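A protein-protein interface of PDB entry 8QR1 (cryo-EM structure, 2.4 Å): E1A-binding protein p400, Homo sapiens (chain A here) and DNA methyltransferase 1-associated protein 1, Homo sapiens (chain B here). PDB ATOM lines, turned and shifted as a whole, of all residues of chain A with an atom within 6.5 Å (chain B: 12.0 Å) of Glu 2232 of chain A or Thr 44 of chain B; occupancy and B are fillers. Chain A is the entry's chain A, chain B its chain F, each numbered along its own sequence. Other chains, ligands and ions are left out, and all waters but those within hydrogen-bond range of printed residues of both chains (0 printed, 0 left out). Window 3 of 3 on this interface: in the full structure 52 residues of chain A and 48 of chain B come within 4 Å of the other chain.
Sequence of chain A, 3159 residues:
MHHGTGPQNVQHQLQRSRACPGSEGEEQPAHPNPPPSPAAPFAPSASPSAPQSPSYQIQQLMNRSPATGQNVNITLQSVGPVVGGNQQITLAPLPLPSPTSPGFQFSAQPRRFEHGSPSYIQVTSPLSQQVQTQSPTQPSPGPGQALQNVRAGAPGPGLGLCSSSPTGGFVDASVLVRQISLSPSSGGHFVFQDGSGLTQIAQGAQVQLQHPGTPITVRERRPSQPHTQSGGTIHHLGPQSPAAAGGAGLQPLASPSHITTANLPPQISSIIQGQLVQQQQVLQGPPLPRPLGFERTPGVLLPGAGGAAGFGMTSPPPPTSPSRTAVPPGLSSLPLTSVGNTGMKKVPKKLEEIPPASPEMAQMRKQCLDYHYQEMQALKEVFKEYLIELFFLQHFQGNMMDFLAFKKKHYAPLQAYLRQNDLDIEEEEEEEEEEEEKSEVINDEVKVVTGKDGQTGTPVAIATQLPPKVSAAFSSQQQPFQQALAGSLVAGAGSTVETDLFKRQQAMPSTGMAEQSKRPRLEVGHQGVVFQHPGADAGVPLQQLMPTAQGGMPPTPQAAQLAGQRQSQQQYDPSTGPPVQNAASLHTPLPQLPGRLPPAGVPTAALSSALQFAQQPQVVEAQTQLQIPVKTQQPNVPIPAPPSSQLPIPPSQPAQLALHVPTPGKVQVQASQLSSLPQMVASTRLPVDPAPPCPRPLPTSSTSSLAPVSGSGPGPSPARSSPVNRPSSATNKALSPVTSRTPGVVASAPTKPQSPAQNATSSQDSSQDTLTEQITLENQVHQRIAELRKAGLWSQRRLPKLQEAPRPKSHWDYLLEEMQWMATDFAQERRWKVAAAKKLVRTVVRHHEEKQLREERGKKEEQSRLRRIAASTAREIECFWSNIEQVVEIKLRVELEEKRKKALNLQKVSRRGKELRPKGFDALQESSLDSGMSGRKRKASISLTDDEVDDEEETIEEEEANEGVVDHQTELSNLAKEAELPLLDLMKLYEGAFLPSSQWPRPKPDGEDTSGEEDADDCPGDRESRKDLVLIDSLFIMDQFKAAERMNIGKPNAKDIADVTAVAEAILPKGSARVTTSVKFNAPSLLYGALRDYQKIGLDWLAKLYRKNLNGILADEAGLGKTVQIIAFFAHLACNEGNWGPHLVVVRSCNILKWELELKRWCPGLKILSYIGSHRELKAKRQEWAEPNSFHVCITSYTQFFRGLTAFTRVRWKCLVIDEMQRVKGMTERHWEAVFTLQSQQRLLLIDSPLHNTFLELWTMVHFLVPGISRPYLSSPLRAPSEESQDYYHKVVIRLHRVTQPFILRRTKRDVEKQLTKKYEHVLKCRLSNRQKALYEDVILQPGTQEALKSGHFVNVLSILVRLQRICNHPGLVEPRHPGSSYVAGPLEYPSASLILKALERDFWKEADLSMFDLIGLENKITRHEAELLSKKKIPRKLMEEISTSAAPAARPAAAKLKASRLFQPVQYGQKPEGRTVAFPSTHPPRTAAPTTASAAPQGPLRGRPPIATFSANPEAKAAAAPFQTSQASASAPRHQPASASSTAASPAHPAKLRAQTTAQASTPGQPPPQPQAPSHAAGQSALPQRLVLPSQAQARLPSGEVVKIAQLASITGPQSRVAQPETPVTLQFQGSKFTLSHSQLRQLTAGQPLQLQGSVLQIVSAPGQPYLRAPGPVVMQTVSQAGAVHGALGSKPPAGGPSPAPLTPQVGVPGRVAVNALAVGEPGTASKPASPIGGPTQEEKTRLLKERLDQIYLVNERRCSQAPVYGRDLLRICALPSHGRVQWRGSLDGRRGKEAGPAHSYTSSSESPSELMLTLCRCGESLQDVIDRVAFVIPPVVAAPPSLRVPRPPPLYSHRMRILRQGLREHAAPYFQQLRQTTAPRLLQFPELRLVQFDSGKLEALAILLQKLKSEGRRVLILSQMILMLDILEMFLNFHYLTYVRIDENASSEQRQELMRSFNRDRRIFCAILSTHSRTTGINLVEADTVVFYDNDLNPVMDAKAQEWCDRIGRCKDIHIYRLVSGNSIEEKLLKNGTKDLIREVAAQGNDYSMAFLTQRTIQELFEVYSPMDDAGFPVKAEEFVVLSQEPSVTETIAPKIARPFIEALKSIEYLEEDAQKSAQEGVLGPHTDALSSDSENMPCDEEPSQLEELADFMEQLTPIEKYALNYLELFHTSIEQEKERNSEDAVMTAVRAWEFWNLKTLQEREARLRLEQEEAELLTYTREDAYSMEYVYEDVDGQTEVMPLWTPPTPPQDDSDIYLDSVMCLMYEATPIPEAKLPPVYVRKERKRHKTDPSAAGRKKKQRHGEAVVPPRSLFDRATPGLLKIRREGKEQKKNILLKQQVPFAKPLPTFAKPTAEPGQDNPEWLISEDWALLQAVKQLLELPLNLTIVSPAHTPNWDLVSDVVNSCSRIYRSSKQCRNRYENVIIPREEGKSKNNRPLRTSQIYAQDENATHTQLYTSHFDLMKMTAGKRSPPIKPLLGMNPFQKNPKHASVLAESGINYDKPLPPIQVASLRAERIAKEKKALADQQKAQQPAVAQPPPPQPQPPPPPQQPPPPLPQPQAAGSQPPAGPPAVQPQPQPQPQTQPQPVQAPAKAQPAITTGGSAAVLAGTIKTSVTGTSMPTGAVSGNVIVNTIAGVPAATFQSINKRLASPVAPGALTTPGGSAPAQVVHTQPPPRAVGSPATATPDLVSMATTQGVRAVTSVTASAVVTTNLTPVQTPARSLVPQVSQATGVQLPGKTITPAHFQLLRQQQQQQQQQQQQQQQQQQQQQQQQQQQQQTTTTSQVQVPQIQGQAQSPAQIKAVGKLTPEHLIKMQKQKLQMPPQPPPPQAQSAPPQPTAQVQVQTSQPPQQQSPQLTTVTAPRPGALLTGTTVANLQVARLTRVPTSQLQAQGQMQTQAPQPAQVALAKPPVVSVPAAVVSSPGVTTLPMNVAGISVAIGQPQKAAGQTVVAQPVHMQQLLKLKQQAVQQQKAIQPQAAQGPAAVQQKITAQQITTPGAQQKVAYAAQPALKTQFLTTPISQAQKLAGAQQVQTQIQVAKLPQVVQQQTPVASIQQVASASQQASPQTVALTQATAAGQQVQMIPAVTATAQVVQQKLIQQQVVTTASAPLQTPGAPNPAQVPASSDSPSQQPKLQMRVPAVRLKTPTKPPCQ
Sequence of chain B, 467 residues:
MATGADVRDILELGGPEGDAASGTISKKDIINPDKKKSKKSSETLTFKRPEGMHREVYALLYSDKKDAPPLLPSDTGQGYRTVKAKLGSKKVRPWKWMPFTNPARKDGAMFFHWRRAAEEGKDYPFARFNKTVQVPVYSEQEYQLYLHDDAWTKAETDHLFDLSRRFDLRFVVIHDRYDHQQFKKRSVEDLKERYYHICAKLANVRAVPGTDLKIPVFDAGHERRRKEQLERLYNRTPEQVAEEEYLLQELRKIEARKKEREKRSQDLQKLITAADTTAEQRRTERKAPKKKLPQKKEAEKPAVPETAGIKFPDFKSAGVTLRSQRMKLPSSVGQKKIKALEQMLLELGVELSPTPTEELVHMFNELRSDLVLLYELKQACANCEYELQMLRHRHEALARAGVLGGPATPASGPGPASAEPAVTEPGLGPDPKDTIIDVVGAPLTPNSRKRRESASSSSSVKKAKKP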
ATOM      1  N   TYR A2229      23.856   6.246  -5.231  1.00  0.00           N
ATOM      2  CA  TYR A2229      22.542   6.330  -5.859  1.00  0.00           C
ATOM      3  C   TYR A2229      22.126   5.018  -6.520  1.00  0.00           C
ATOM      4  O   TYR A2229      21.422   5.030  -7.534  1.00  0.00           O
ATOM      5  CB  TYR A2229      22.530   7.480  -6.862  1.00  0.00           C
ATOM      6  CG  TYR A2229      23.042   8.776  -6.274  1.00  0.00           C
ATOM      7  CD1 TYR A2229      22.220   9.581  -5.504  1.00  0.00           C
ATOM      8  CD2 TYR A2229      24.349   9.184  -6.474  1.00  0.00           C
ATOM      9  CE1 TYR A2229      22.684  10.760  -4.959  1.00  0.00           C
ATOM     10  CE2 TYR A2229      24.821  10.360  -5.932  1.00  0.00           C
ATOM     11  CZ  TYR A2229      23.984  11.144  -5.175  1.00  0.00           C
ATOM     12  OH  TYR A2229      24.449  12.317  -4.633  1.00  0.00           O
ATOM     13  N   SER A2230      22.549   3.881  -5.957  1.00  0.00           N
ATOM     14  CA  SER A2230      22.061   2.589  -6.433  1.00  0.00           C
ATOM     15  C   SER A2230      20.632   2.341  -5.976  1.00  0.00           C
ATOM     16  O   SER A2230      19.811   1.814  -6.737  1.00  0.00           O
ATOM     17  CB  SER A2230      22.963   1.464  -5.930  1.00  0.00           C
ATOM     18  OG  SER A2230      22.451   0.200  -6.306  1.00  0.00           O
ATOM     19  N   MET A2231      20.337   2.672  -4.715  1.00  0.00           N
ATOM     20  CA  MET A2231      19.030   2.506  -4.083  1.00  0.00           C
ATOM     21  C   MET A2231      18.656   1.049  -3.805  1.00  0.00           C
ATOM     22  O   MET A2231      17.571   0.794  -3.273  1.00  0.00           O
ATOM     23  CB  MET A2231      17.933   3.160  -4.933  1.00  0.00           C
ATOM     24  N   GLU A2232      19.524   0.087  -4.138  1.00  0.00           N
ATOM     25  CA  GLU A2232      19.172  -1.317  -3.964  1.00  0.00           C
ATOM     26  C   GLU A2232      19.421  -1.788  -2.536  1.00  0.00           C
ATOM     27  O   GLU A2232      18.463  -1.968  -1.778  1.00  0.00           O
ATOM     28  CB  GLU A2232      19.974  -2.172  -4.944  1.00  0.00           C
ATOM     29  CG  GLU A2232      19.594  -1.972  -6.397  1.00  0.00           C
ATOM     30  CD  GLU A2232      20.421  -2.830  -7.330  1.00  0.00           C
ATOM     31  OE1 GLU A2232      21.046  -3.794  -6.846  1.00  0.00           O
ATOM     32  OE2 GLU A2232      20.448  -2.543  -8.546  1.00  0.00           O
ATOM     33  N   TYR A2233      20.705  -1.912  -2.160  1.00  0.00           N
ATOM     34  CA  TYR A2233      21.193  -2.251  -0.820  1.00  0.00           C
ATOM     35  C   TYR A2233      20.379  -3.327  -0.104  1.00  0.00           C
ATOM     36  O   TYR A2233      19.716  -3.042   0.897  1.00  0.00           O
ATOM     37  CB  TYR A2233      21.276  -0.984   0.028  1.00  0.00           C
ATOM     38  CG  TYR A2233      22.460  -0.119  -0.318  1.00  0.00           C
ATOM     39  CD1 TYR A2233      22.351   0.921  -1.226  1.00  0.00           C
ATOM     40  CD2 TYR A2233      23.696  -0.354   0.263  1.00  0.00           C
ATOM     41  CE1 TYR A2233      23.437   1.707  -1.536  1.00  0.00           C
ATOM     42  CE2 TYR A2233      24.784   0.425  -0.043  1.00  0.00           C
ATOM     43  CZ  TYR A2233      24.651   1.456  -0.938  1.00  0.00           C
ATOM     44  OH  TYR A2233      25.742   2.230  -1.246  1.00  0.00           O
ATOM     45  N   VAL A2234      20.394  -4.551  -0.630  1.00  0.00           N
ATOM     46  CA  VAL A2234      19.474  -5.605  -0.218  1.00  0.00           C
ATOM     47  C   VAL A2234      20.198  -6.631   0.642  1.00  0.00           C
ATOM     48  O   VAL A2234      21.426  -6.764   0.599  1.00  0.00           O
ATOM     49  CB  VAL A2234      18.808  -6.295  -1.431  1.00  0.00           C
ATOM     50  CG1 VAL A2234      18.041  -5.278  -2.261  1.00  0.00           C
ATOM     51  CG2 VAL A2234      19.820  -7.064  -2.286  1.00  0.00           C
ATOM     52  N   TYR A2235      19.408  -7.352   1.436  1.00  0.00           N
ATOM     53  CA  TYR A2235      19.841  -8.493   2.229  1.00  0.00           C
ATOM     54  C   TYR A2235      18.899  -9.656   1.960  1.00  0.00           C
ATOM     55  O   TYR A2235      17.705  -9.455   1.735  1.00  0.00           O
ATOM     56  CB  TYR A2235      19.843  -8.157   3.728  1.00  0.00           C
ATOM     57  CG  TYR A2235      20.147  -9.321   4.645  1.00  0.00           C
ATOM     58  CD1 TYR A2235      21.289 -10.088   4.475  1.00  0.00           C
ATOM     59  CD2 TYR A2235      19.291  -9.648   5.684  1.00  0.00           C
ATOM     60  CE1 TYR A2235      21.566 -11.150   5.308  1.00  0.00           C
ATOM     61  CE2 TYR A2235      19.561 -10.707   6.523  1.00  0.00           C
ATOM     62  CZ  TYR A2235      20.699 -11.454   6.332  1.00  0.00           C
ATOM     63  OH  TYR A2235      20.971 -12.512   7.165  1.00  0.00           O
ATOM     64  N   GLU A2243      15.215  -8.123   2.516  1.00  0.00           N
ATOM     65  CA  GLU A2243      15.058  -6.817   3.138  1.00  0.00           C
ATOM     66  C   GLU A2243      15.794  -5.773   2.312  1.00  0.00           C
ATOM     67  O   GLU A2243      16.798  -6.072   1.662  1.00  0.00           O
ATOM     68  CB  GLU A2243      15.606  -6.800   4.568  1.00  0.00           C
ATOM     69  CG  GLU A2243      15.087  -7.910   5.461  1.00  0.00           C
ATOM     70  CD  GLU A2243      15.548  -7.768   6.900  1.00  0.00           C
ATOM     71  OE1 GLU A2243      16.156  -6.730   7.238  1.00  0.00           O
ATOM     72  OE2 GLU A2243      15.302  -8.697   7.697  1.00  0.00           O
ATOM     73  N   VAL A2244      15.277  -4.547   2.350  1.00  0.00           N
ATOM     74  CA  VAL A2244      15.889  -3.391   1.704  1.00  0.00           C
ATOM     75  C   VAL A2244      16.430  -2.475   2.789  1.00  0.00           C
ATOM     76  O   VAL A2244      15.770  -2.256   3.813  1.00  0.00           O
ATOM     77  CB  VAL A2244      14.884  -2.648   0.807  1.00  0.00           C
ATOM     78  CG1 VAL A2244      15.527  -1.398   0.220  1.00  0.00           C
ATOM     79  CG2 VAL A2244      14.380  -3.560  -0.304  1.00  0.00           C
ATOM     80  N   MET A2245      17.630  -1.953   2.575  1.00  0.00           N
ATOM     81  CA  MET A2245      18.253  -1.089   3.563  1.00  0.00           C
ATOM     82  C   MET A2245      17.462   0.214   3.684  1.00  0.00           C
ATOM     83  O   MET A2245      17.143   0.828   2.656  1.00  0.00           O
ATOM     84  CB  MET A2245      19.692  -0.786   3.169  1.00  0.00           C
ATOM     85  CG  MET A2245      20.507  -0.145   4.261  1.00  0.00           C
ATOM     86  SD  MET A2245      22.275  -0.210   3.938  1.00  0.00           S
ATOM     87  CE  MET A2245      22.899   0.077   5.583  1.00  0.00           C
ATOM     88  N   THR B  44      21.653  -6.333  -6.817  1.00  0.00           N
ATOM     89  CA  THR B  44      23.092  -6.232  -7.196  1.00  0.00           C
ATOM     90  C   THR B  44      23.943  -5.911  -5.977  1.00  0.00           C
ATOM     91  O   THR B  44      24.863  -6.655  -5.635  1.00  0.00           O
ATOM     92  CB  THR B  44      23.333  -5.146  -8.269  1.00  0.00           C
ATOM     93  OG1 THR B  44      23.256  -3.849  -7.665  1.00  0.00           O
ATOM     94  CG2 THR B  44      22.315  -5.243  -9.396  1.00  0.00           C
ATOM     95  N   LEU B  45      23.621  -4.800  -5.320  1.00  0.00           N
ATOM     96  CA  LEU B  45      24.409  -4.274  -4.216  1.00  0.00           C
ATOM     97  C   LEU B  45      23.892  -4.834  -2.898  1.00  0.00           C
ATOM     98  O   LEU B  45      22.677  -4.902  -2.682  1.00  0.00           O
ATOM     99  CB  LEU B  45      24.359  -2.747  -4.213  1.00  0.00           C
ATOM    100  CG  LEU B  45      25.252  -1.944  -3.261  1.00  0.00           C
ATOM    101  CD1 LEU B  45      26.692  -2.415  -3.228  1.00  0.00           C
ATOM    102  CD2 LEU B  45      25.206  -0.487  -3.670  1.00  0.00           C
ATOM    103  N   THR B  46      24.817  -5.212  -2.021  1.00  0.00           N
ATOM    104  CA  THR B  46      24.537  -6.053  -0.868  1.00  0.00           C
ATOM    105  C   THR B  46      24.724  -5.273   0.425  1.00  0.00           C
ATOM    106  O   THR B  46      25.692  -4.519   0.568  1.00  0.00           O
ATOM    107  CB  THR B  46      25.455  -7.279  -0.870  1.00  0.00           C
ATOM    108  OG1 THR B  46      25.307  -7.988  -2.107  1.00  0.00           O
ATOM    109  CG2 THR B  46      25.136  -8.213   0.289  1.00  0.00           C
ATOM    110  N   PHE B  47      23.785  -5.450   1.348  1.00  0.00           N
ATOM    111  CA  PHE B  47      23.956  -5.107   2.749  1.00  0.00           C
ATOM    112  C   PHE B  47      23.587  -6.336   3.564  1.00  0.00           C
ATOM    113  O   PHE B  47      22.854  -7.211   3.097  1.00  0.00           O
ATOM    114  CB  PHE B  47      23.120  -3.874   3.135  1.00  0.00           C
ATOM    115  CG  PHE B  47      21.908  -4.169   3.972  1.00  0.00           C
ATOM    116  CD1 PHE B  47      20.710  -4.518   3.383  1.00  0.00           C
ATOM    117  CD2 PHE B  47      21.953  -4.036   5.347  1.00  0.00           C
ATOM    118  CE1 PHE B  47      19.592  -4.764   4.151  1.00  0.00           C
ATOM    119  CE2 PHE B  47      20.838  -4.284   6.116  1.00  0.00           C
ATOM    120  CZ  PHE B  47      19.659  -4.647   5.517  1.00  0.00           C
ATOM    121  N   LYS B  48      24.124  -6.406   4.779  1.00  0.00           N
ATOM    122  CA  LYS B  48      24.244  -7.656   5.517  1.00  0.00           C
ATOM    123  C   LYS B  48      23.717  -7.477   6.934  1.00  0.00           C
ATOM    124  O   LYS B  48      24.120  -6.545   7.636  1.00  0.00           O
ATOM    125  CB  LYS B  48      25.707  -8.099   5.522  1.00  0.00           C
ATOM    126  CG  LYS B  48      25.962  -9.522   5.945  1.00  0.00           C
ATOM    127  CD  LYS B  48      27.442  -9.767   6.272  1.00  0.00           C
ATOM    128  CE  LYS B  48      28.383  -9.549   5.084  1.00  0.00           C
ATOM    129  NZ  LYS B  48      28.129 -10.521   3.984  1.00  0.00           N
ATOM    130  N   ARG B  49      22.811  -8.366   7.337  1.00  0.00           N
ATOM    131  CA  ARG B  49      22.205  -8.355   8.671  1.00  0.00           C
ATOM    132  C   ARG B  49      22.182  -9.792   9.180  1.00  0.00           C
ATOM    133  O   ARG B  49      21.117 -10.393   9.370  1.00  0.00           O
ATOM    134  CB  ARG B  49      20.807  -7.733   8.617  1.00  0.00           C
ATOM    135  CG  ARG B  49      20.304  -7.184   9.949  1.00  0.00           C
ATOM    136  CD  ARG B  49      19.089  -6.275   9.785  1.00  0.00           C
ATOM    137  NE  ARG B  49      17.832  -7.011   9.717  1.00  0.00           N
ATOM    138  CZ  ARG B  49      17.154  -7.475  10.760  1.00  0.00           C
ATOM    139  NH1 ARG B  49      17.589  -7.330  12.003  1.00  0.00           N
ATOM    140  NH2 ARG B  49      16.000  -8.101  10.553  1.00  0.00           N
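The backbone NH (N) of Tyr 2235 of chain A sits at hydrogen-bond distance from the backbone carbonyl oxygen (O) of Glu 2243 of chain A.
The backbone carbonyl oxygen (O) of Tyr 2233 of chain A lies within hydrogen-bond range of the backbone NH (N) of Met 2245 of chain A, at 2.9 Å.
Among the printed residues, pairs that only touch across the chains: Ser 2230 of chain A with Leu 45 of chain B (3.7 Å), Tyr 2233 of chain A with Leu 45 of chain B (3.4 Å), Tyr 2233 of chain A with Phe 47 of chain B (3.1 Å), Val 2234 of chain A with Thr 46 of chain B (3.5 Å), Tyr 2235 of chain A with Phe 47 of chain B (3.2 Å), Tyr 2235 of chain A with Lys 48 of chain B (3.97 Å), Glu 2243 of chain A with Phe 47 of chain B (3.96 Å) and Met 2245 of chain A with Phe 47 of chain B (3.8 Å).
OE2 of Glu 2243 of chain A is in salt-bridge range of NH2 of Arg 49 of chain B (3.0 Å).
The side-chain hydroxyl (OH) of Tyr 2235 of chain A lies within hydrogen-bond range of the backbone carbonyl oxygen (O) of Arg 49 of chain B (3.1 Å).
The backbone NH of Val 2234 of chain A lies within hydrogen-bond range of the backbone carbonyl oxygen of Leu 45 of chain B (3.1 Å).
The backbone carbonyl oxygen of Val 2234 of chain A lies within hydrogen-bond range of the backbone NH of Phe 47 of chain B (2.8 Å).
The side-chain carboxylate of Glu 2232 of chain A lies within hydrogen-bond range of the backbone NH of Thr 44 of chain B (2.6 Å).
The side-chain carboxylate of Glu 2232 of chain A lies within hydrogen-bond range of the backbone NH of Leu 45 of chain B.
Along chain A the printed residues that touch a printed residue of chain B span positions 2230 to 2245.
Tyr 2229 of chain A touches none of the printed residues of chain B.
Of chain B, only Leu 45 comes within 4 Å of Ser 2230 of chain A.
No residue of chain B comes within 4 Å of Met 2231 of chain A.
Glu 2232 of chain A touches just these residues of chain B: Thr 44 (2.4 Å) and Leu 45 (3.2 Å).
Of chain B, only Leu 45 and Phe 47 come within 4 Å of Tyr 2233 of chain A.
Printed residues of chain B within 4 Å of Val 2234 of chain A: Leu 45, Thr 46 and Phe 47.
Printed residues of chain B within 4 Å of Tyr 2235 of chain A: Phe 47 (3.2 Å), Lys 48 (3.97 Å) and Arg 49 (3.1 Å).
Printed residues of chain B within 4 Å of Glu 2243 of chain A: Phe 47 and Arg 49.
No residue of chain B comes within 4 Å of Val 2244 of chain A.
Of the printed residues of chain B, Met 2245 of chain A touches Phe 47.
Of the printed residues of chain A, Thr 44 of chain B touches Glu 2232 (2.4 Å).
Printed residues of chain A within 4 Å of Thr 46 of chain B: Val 2234 (3.5 Å).
Of the printed residues of chain A, Arg 49 of chain B touches Tyr 2235 and Glu 2243.
The nearest residue of chain A that does not touch Thr 44 of chain B is Ser 2230 of chain A (4.3 Å).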
